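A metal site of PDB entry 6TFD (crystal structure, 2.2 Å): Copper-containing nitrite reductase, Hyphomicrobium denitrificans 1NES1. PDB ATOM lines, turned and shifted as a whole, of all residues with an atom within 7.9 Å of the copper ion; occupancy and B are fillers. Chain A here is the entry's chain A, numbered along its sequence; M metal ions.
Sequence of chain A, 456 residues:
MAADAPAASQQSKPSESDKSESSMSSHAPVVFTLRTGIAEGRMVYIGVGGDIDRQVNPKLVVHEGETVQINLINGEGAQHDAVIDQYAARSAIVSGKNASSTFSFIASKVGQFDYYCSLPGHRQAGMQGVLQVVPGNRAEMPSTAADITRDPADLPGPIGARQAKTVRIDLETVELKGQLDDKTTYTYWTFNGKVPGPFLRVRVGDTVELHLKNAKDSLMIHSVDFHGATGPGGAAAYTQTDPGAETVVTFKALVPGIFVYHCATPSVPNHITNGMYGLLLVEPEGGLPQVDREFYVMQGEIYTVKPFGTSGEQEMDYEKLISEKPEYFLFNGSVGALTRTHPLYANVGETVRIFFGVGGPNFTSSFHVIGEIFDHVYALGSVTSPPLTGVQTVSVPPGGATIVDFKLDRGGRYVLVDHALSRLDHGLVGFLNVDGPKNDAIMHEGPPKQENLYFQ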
ATOM      1  N   THR A 173      14.418  24.951  23.980  1.00  0.00           N
ATOM      2  CA  THR A 173      13.728  24.138  25.021  1.00  0.00           C
ATOM      3  C   THR A 173      13.049  25.110  25.997  1.00  0.00           C
ATOM      4  O   THR A 173      13.775  25.856  26.678  1.00  0.00           O
ATOM      5  CB  THR A 173      14.708  23.148  25.644  1.00  0.00           C
ATOM      6  OG1 THR A 173      15.854  23.876  26.113  1.00  0.00           O
ATOM      7  CG2 THR A 173      15.140  22.087  24.657  1.00  0.00           C
ATOM      8  N   VAL A 174      11.710  25.084  26.062  1.00  0.00           N
ATOM      9  CA  VAL A 174      10.881  26.080  26.789  1.00  0.00           C
ATOM     10  C   VAL A 174       9.891  25.330  27.676  1.00  0.00           C
ATOM     11  O   VAL A 174       9.136  24.493  27.130  1.00  0.00           O
ATOM     12  CB  VAL A 174      10.125  26.997  25.805  1.00  0.00           C
ATOM     13  CG1 VAL A 174       9.309  28.047  26.536  1.00  0.00           C
ATOM     14  CG2 VAL A 174      11.038  27.642  24.774  1.00  0.00           C
ATOM     15  N   GLU A 175       9.910  25.612  28.995  1.00  0.00           N
ATOM     16  CA  GLU A 175       8.945  25.119  30.018  1.00  0.00           C
ATOM     17  C   GLU A 175       7.886  26.211  30.224  1.00  0.00           C
ATOM     18  O   GLU A 175       8.251  27.366  30.358  1.00  0.00           O
ATOM     19  CB  GLU A 175       9.623  24.789  31.345  1.00  0.00           C
ATOM     20  CG  GLU A 175      10.827  23.864  31.225  1.00  0.00           C
ATOM     21  CD  GLU A 175      11.682  23.838  32.486  1.00  0.00           C
ATOM     22  OE1 GLU A 175      12.739  23.126  32.522  1.00  0.00           O
ATOM     23  OE2 GLU A 175      11.313  24.576  33.421  1.00  0.00           O
ATOM     24  N   TRP A 189       6.813  20.919  28.954  1.00  0.00           N
ATOM     25  CA  TRP A 189       8.202  21.106  28.485  1.00  0.00           C
ATOM     26  C   TRP A 189       8.159  20.891  26.980  1.00  0.00           C
ATOM     27  O   TRP A 189       7.562  19.873  26.558  1.00  0.00           O
ATOM     28  CB  TRP A 189       9.171  20.138  29.184  1.00  0.00           C
ATOM     29  CG  TRP A 189       9.184  20.225  30.685  1.00  0.00           C
ATOM     30  CD1 TRP A 189       8.568  21.186  31.438  1.00  0.00           C
ATOM     31  CD2 TRP A 189       9.840  19.345  31.628  1.00  0.00           C
ATOM     32  NE1 TRP A 189       8.811  20.972  32.766  1.00  0.00           N
ATOM     33  CE2 TRP A 189       9.568  19.847  32.912  1.00  0.00           C
ATOM     34  CE3 TRP A 189      10.599  18.179  31.511  1.00  0.00           C
ATOM     35  CZ2 TRP A 189      10.040  19.233  34.076  1.00  0.00           C
ATOM     36  CZ3 TRP A 189      11.063  17.559  32.653  1.00  0.00           C
ATOM     37  CH2 TRP A 189      10.784  18.079  33.922  1.00  0.00           C
ATOM     38  N   THR A 190       8.702  21.830  26.204  1.00  0.00           N
ATOM     39  CA  THR A 190       8.570  21.821  24.724  1.00  0.00           C
ATOM     40  C   THR A 190       9.894  22.143  24.006  1.00  0.00           C
ATOM     41  O   THR A 190      10.877  22.607  24.621  1.00  0.00           O
ATOM     42  CB  THR A 190       7.505  22.826  24.287  1.00  0.00           C
ATOM     43  OG1 THR A 190       8.044  24.126  24.561  1.00  0.00           O
ATOM     44  CG2 THR A 190       6.180  22.629  24.982  1.00  0.00           C
ATOM     45  N   PHE A 191       9.897  21.832  22.707  1.00  0.00           N
ATOM     46  CA  PHE A 191      10.822  22.380  21.696  1.00  0.00           C
ATOM     47  C   PHE A 191      10.054  23.548  21.070  1.00  0.00           C
ATOM     48  O   PHE A 191       9.040  23.258  20.436  1.00  0.00           O
ATOM     49  CB  PHE A 191      11.191  21.291  20.679  1.00  0.00           C
ATOM     50  CG  PHE A 191      12.075  20.198  21.215  1.00  0.00           C
ATOM     51  CD1 PHE A 191      13.365  20.466  21.626  1.00  0.00           C
ATOM     52  CD2 PHE A 191      11.622  18.899  21.306  1.00  0.00           C
ATOM     53  CE1 PHE A 191      14.186  19.445  22.091  1.00  0.00           C
ATOM     54  CE2 PHE A 191      12.422  17.882  21.797  1.00  0.00           C
ATOM     55  CZ  PHE A 191      13.707  18.153  22.196  1.00  0.00           C
ATOM     56  N   ASN A 214      18.648  26.412  25.688  1.00  0.00           N
ATOM     57  CA  ASN A 214      17.766  26.209  26.864  1.00  0.00           C
ATOM     58  C   ASN A 214      17.365  27.594  27.339  1.00  0.00           C
ATOM     59  O   ASN A 214      18.288  28.365  27.685  1.00  0.00           O
ATOM     60  CB  ASN A 214      18.437  25.419  27.982  1.00  0.00           C
ATOM     61  CG  ASN A 214      17.456  24.712  28.894  1.00  0.00           C
ATOM     62  OD1 ASN A 214      16.258  24.941  28.820  1.00  0.00           O
ATOM     63  ND2 ASN A 214      17.967  23.828  29.731  1.00  0.00           N
ATOM     64  N   MET A 220      15.112  22.982  34.381  1.00  0.00           N
ATOM     65  CA  MET A 220      15.781  21.684  34.100  1.00  0.00           C
ATOM     66  C   MET A 220      16.760  21.826  32.927  1.00  0.00           C
ATOM     67  O   MET A 220      16.542  22.663  32.021  1.00  0.00           O
ATOM     68  CB  MET A 220      14.761  20.585  33.770  1.00  0.00           C
ATOM     69  CG  MET A 220      13.451  20.692  34.548  1.00  0.00           C
ATOM     70  SD  MET A 220      13.503  20.061  36.243  1.00  0.00           S
ATOM     71  CE  MET A 220      15.092  20.641  36.802  1.00  0.00           C
ATOM     72  N   ILE A 221      17.813  21.003  32.961  1.00  0.00           N
ATOM     73  CA  ILE A 221      18.634  20.638  31.782  1.00  0.00           C
ATOM     74  C   ILE A 221      17.710  20.014  30.719  1.00  0.00           C
ATOM     75  O   ILE A 221      16.743  19.269  31.067  1.00  0.00           O
ATOM     76  CB  ILE A 221      19.803  19.717  32.217  1.00  0.00           C
ATOM     77  CG1 ILE A 221      20.777  20.453  33.156  1.00  0.00           C
ATOM     78  CG2 ILE A 221      20.527  19.111  31.017  1.00  0.00           C
ATOM     79  CD1 ILE A 221      21.620  19.543  34.065  1.00  0.00           C
ATOM     80  N   HIS A 222      17.970  20.311  29.441  1.00  0.00           N
ATOM     81  CA  HIS A 222      17.280  19.685  28.277  1.00  0.00           C
ATOM     82  C   HIS A 222      18.294  19.287  27.212  1.00  0.00           C
ATOM     83  O   HIS A 222      19.477  19.696  27.290  1.00  0.00           O
ATOM     84  CB  HIS A 222      16.179  20.617  27.752  1.00  0.00           C
ATOM     85  CG  HIS A 222      15.120  20.860  28.762  1.00  0.00           C
ATOM     86  ND1 HIS A 222      14.086  19.977  28.974  1.00  0.00           N
ATOM     87  CD2 HIS A 222      14.920  21.895  29.599  1.00  0.00           C
ATOM     88  CE1 HIS A 222      13.295  20.456  29.920  1.00  0.00           C
ATOM     89  NE2 HIS A 222      13.784  21.631  30.320  1.00  0.00           N
ATOM     90  N   SER A 223      17.845  18.492  26.251  1.00  0.00           N
ATOM     91  CA  SER A 223      18.713  17.791  25.280  1.00  0.00           C
ATOM     92  C   SER A 223      17.874  17.428  24.064  1.00  0.00           C
ATOM     93  O   SER A 223      16.688  17.812  24.026  1.00  0.00           O
ATOM     94  CB  SER A 223      19.318  16.572  25.919  1.00  0.00           C
ATOM     95  OG  SER A 223      18.287  15.636  26.225  1.00  0.00           O
ATOM     96  N   VAL A 224      18.465  16.711  23.103  1.00  0.00           N
ATOM     97  CA  VAL A 224      17.700  16.067  21.998  1.00  0.00           C
ATOM     98  C   VAL A 224      18.479  14.847  21.509  1.00  0.00           C
ATOM     99  O   VAL A 224      19.692  14.993  21.288  1.00  0.00           O
ATOM    100  CB  VAL A 224      17.416  17.066  20.860  1.00  0.00           C
ATOM    101  CG1 VAL A 224      18.694  17.625  20.254  1.00  0.00           C
ATOM    102  CG2 VAL A 224      16.515  16.450  19.790  1.00  0.00           C
ATOM    103  N   GLN A 240      23.382  18.148  26.106  1.00  0.00           N
ATOM    104  CA  GLN A 240      22.924  18.378  27.511  1.00  0.00           C
ATOM    105  C   GLN A 240      23.182  19.854  27.842  1.00  0.00           C
ATOM    106  O   GLN A 240      24.344  20.204  28.030  1.00  0.00           O
ATOM    107  CB  GLN A 240      23.603  17.418  28.474  1.00  0.00           C
ATOM    108  CG  GLN A 240      23.302  15.951  28.173  1.00  0.00           C
ATOM    109  CD  GLN A 240      21.853  15.569  28.372  1.00  0.00           C
ATOM    110  OE1 GLN A 240      21.126  16.150  29.179  1.00  0.00           O
ATOM    111  NE2 GLN A 240      21.438  14.562  27.625  1.00  0.00           N
ATOM    112  N   HIS A 262      13.379  13.385  20.410  1.00  0.00           N
ATOM    113  CA  HIS A 262      12.840  13.626  21.773  1.00  0.00           C
ATOM    114  C   HIS A 262      13.954  14.117  22.686  1.00  0.00           C
ATOM    115  O   HIS A 262      15.139  13.832  22.371  1.00  0.00           O
ATOM    116  CB  HIS A 262      12.169  12.356  22.330  1.00  0.00           C
ATOM    117  CG  HIS A 262      13.058  11.169  22.487  1.00  0.00           C
ATOM    118  ND1 HIS A 262      13.963  11.041  23.548  1.00  0.00           N
ATOM    119  CD2 HIS A 262      13.175  10.034  21.774  1.00  0.00           C
ATOM    120  CE1 HIS A 262      14.592   9.874  23.463  1.00  0.00           C
ATOM    121  NE2 HIS A 262      14.135   9.248  22.375  1.00  0.00           N
ATOM    122  N   CYS A 263      13.600  14.830  23.776  1.00  0.00           N
ATOM    123  CA  CYS A 263      14.555  15.218  24.837  1.00  0.00           C
ATOM    124  C   CYS A 263      15.113  13.933  25.436  1.00  0.00           C
ATOM    125  O   CYS A 263      14.414  12.919  25.396  1.00  0.00           O
ATOM    126  CB  CYS A 263      13.965  16.123  25.930  1.00  0.00           C
ATOM    127  SG  CYS A 263      15.129  16.554  27.252  1.00  0.00           S
ATOM    128  N   ALA A 264      16.341  13.972  25.937  1.00  0.00           N
ATOM    129  CA  ALA A 264      17.076  12.790  26.443  1.00  0.00           C
ATOM    130  C   ALA A 264      17.849  13.191  27.700  1.00  0.00           C
ATOM    131  O   ALA A 264      18.970  12.744  27.859  1.00  0.00           O
ATOM    132  CB  ALA A 264      18.015  12.261  25.385  1.00  0.00           C
ATOM    133  N   THR A 265      17.258  14.045  28.520  1.00  0.00           N
ATOM    134  CA  THR A 265      17.739  14.342  29.894  1.00  0.00           C
ATOM    135  C   THR A 265      16.882  13.529  30.854  1.00  0.00           C
ATOM    136  O   THR A 265      15.658  13.502  30.717  1.00  0.00           O
ATOM    137  CB  THR A 265      17.694  15.845  30.180  1.00  0.00           C
ATOM    138  OG1 THR A 265      18.377  16.526  29.140  1.00  0.00           O
ATOM    139  CG2 THR A 265      18.324  16.179  31.509  1.00  0.00           C
ATOM    140  N   PRO A 266      17.497  12.843  31.846  1.00  0.00           N
ATOM    141  CA  PRO A 266      16.724  12.117  32.863  1.00  0.00           C
ATOM    142  C   PRO A 266      15.848  13.050  33.695  1.00  0.00           C
ATOM    143  O   PRO A 266      16.288  14.148  34.034  1.00  0.00           O
ATOM    144  CB  PRO A 266      17.818  11.545  33.779  1.00  0.00           C
ATOM    145  CG  PRO A 266      19.070  11.507  32.912  1.00  0.00           C
ATOM    146  CD  PRO A 266      18.949  12.723  32.022  1.00  0.00           C
ATOM    147  N   SER A 267      14.606  12.650  34.039  1.00  0.00           N
ATOM    148  CA  SER A 267      13.914  11.440  33.620  1.00  0.00           C
ATOM    149  C   SER A 267      13.453  11.618  32.173  1.00  0.00           C
ATOM    150  O   SER A 267      12.674  12.558  31.889  1.00  0.00           O
ATOM    151  CB  SER A 267      12.725  11.155  34.540  1.00  0.00           C
ATOM    152  OG  SER A 267      11.883  10.121  34.042  1.00  0.00           O
ATOM    153  N   VAL A 268      13.917  10.747  31.274  1.00  0.00           N
ATOM    154  CA  VAL A 268      13.576  10.821  29.823  1.00  0.00           C
ATOM    155  C   VAL A 268      12.077  10.626  29.694  1.00  0.00           C
ATOM    156  O   VAL A 268      11.419  11.446  29.053  1.00  0.00           O
ATOM    157  CB  VAL A 268      14.407   9.835  28.969  1.00  0.00           C
ATOM    158  CG1 VAL A 268      13.984   9.845  27.500  1.00  0.00           C
ATOM    159  CG2 VAL A 268      15.901  10.097  29.106  1.00  0.00           C
ATOM    160  N   ASN A 270       9.802  11.458  31.749  1.00  0.00           N
ATOM    161  CA  ASN A 270       9.185  12.706  32.282  1.00  0.00           C
ATOM    162  C   ASN A 270       9.301  13.779  31.203  1.00  0.00           C
ATOM    163  O   ASN A 270       8.252  14.408  30.871  1.00  0.00           O
ATOM    164  CB  ASN A 270       9.837  13.149  33.596  1.00  0.00           C
ATOM    165  CG  ASN A 270       9.179  14.341  34.265  1.00  0.00           C
ATOM    166  OD1 ASN A 270       7.995  14.622  34.080  1.00  0.00           O
ATOM    167  ND2 ASN A 270       9.937  15.027  35.089  1.00  0.00           N
ATOM    168  N   HIS A 271      10.507  13.979  30.657  1.00  0.00           N
ATOM    169  CA  HIS A 271      10.746  14.983  29.599  1.00  0.00           C
ATOM    170  C   HIS A 271       9.822  14.684  28.393  1.00  0.00           C
ATOM    171  O   HIS A 271       9.224  15.661  27.873  1.00  0.00           O
ATOM    172  CB  HIS A 271      12.236  15.069  29.256  1.00  0.00           C
ATOM    173  CG  HIS A 271      13.047  15.741  30.294  1.00  0.00           C
ATOM    174  ND1 HIS A 271      13.511  17.031  30.154  1.00  0.00           N
ATOM    175  CD2 HIS A 271      13.494  15.321  31.499  1.00  0.00           C
ATOM    176  CE1 HIS A 271      14.184  17.382  31.230  1.00  0.00           C
ATOM    177  NE2 HIS A 271      14.204  16.355  32.071  1.00  0.00           N
ATOM    178  N   ILE A 272       9.677  13.412  27.998  1.00  0.00           N
ATOM    179  CA  ILE A 272       8.797  13.043  26.846  1.00  0.00           C
ATOM    180  C   ILE A 272       7.334  13.326  27.201  1.00  0.00           C
ATOM    181  O   ILE A 272       6.732  14.028  26.418  1.00  0.00           O
ATOM    182  CB  ILE A 272       8.988  11.603  26.332  1.00  0.00           C
ATOM    183  CG1 ILE A 272      10.316  11.408  25.606  1.00  0.00           C
ATOM    184  CG2 ILE A 272       7.845  11.222  25.403  1.00  0.00           C
ATOM    185  CD1 ILE A 272      10.742   9.943  25.497  1.00  0.00           C
ATOM    186  N   ASN A 274       5.863  15.355  29.173  1.00  0.00           N
ATOM    187  CA  ASN A 274       5.607  16.817  29.312  1.00  0.00           C
ATOM    188  C   ASN A 274       5.616  17.517  27.943  1.00  0.00           C
ATOM    189  O   ASN A 274       5.198  18.711  27.906  1.00  0.00           O
ATOM    190  CB  ASN A 274       6.581  17.477  30.276  1.00  0.00           C
ATOM    191  CG  ASN A 274       6.341  17.153  31.730  1.00  0.00           C
ATOM    192  OD1 ASN A 274       7.153  17.522  32.574  1.00  0.00           O
ATOM    193  ND2 ASN A 274       5.286  16.436  32.052  1.00  0.00           N
ATOM    194  N   GLY A 275       6.072  16.838  26.861  1.00  0.00           N
ATOM    195  CA  GLY A 275       5.821  17.233  25.465  1.00  0.00           C
ATOM    196  C   GLY A 275       7.048  17.353  24.563  1.00  0.00           C
ATOM    197  O   GLY A 275       6.872  17.843  23.440  1.00  0.00           O
ATOM    198  N   MET A 276       8.234  16.896  24.980  1.00  0.00           N
ATOM    199  CA  MET A 276       9.504  17.096  24.229  1.00  0.00           C
ATOM    200  C   MET A 276       9.713  15.941  23.229  1.00  0.00           C
ATOM    201  O   MET A 276      10.691  15.176  23.371  1.00  0.00           O
ATOM    202  CB  MET A 276      10.692  17.231  25.205  1.00  0.00           C
ATOM    203  CG  MET A 276      10.510  18.341  26.251  1.00  0.00           C
ATOM    204  SD  MET A 276      12.016  18.874  27.145  1.00  0.00           S
ATOM    205  CE  MET A 276      12.762  19.831  25.829  1.00  0.00           C
HETATM  206 CU    CU M   1      13.896  18.034  28.359  1.00  0.00          CU
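Of the 26 residues printed, 4 come within 4 Å of the copper ion. The nearest printed residue that does not touch the copper ion is Ile 221 (4.1 Å).
The backbone carbonyl oxygen (O) of Met 220 lies close to a ring nitrogen (NE2) of His 222, at 3.4 Å. The side-chain carboxylate of Glu 175 is in hydrogen-bond range of a ring nitrogen (NE2) of His 222 (2.9 Å). O of Thr 265 sits close to NE2 of His 271 (3.5 Å). The side-chain sulfur (SG) of Cys 263 sits close to the side-chain hydroxyl (OG) of Ser 223 (3.4 Å). The side-chain sulfur (SG) of Cys 263 sits close to the backbone NH (N) of Thr 265 (3.5 Å). O of Trp 189 lies close to N of Met 276, 3.4 Å away.
ND1 of His 222 is bound to the copper ion, 2.0 Å away. A ring nitrogen (ND1) of His 271 binds the copper ion (2.1 Å). SG of Cys 263 is bound to the copper ion (2.2 Å). SD of Met 276 binds the copper ion.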
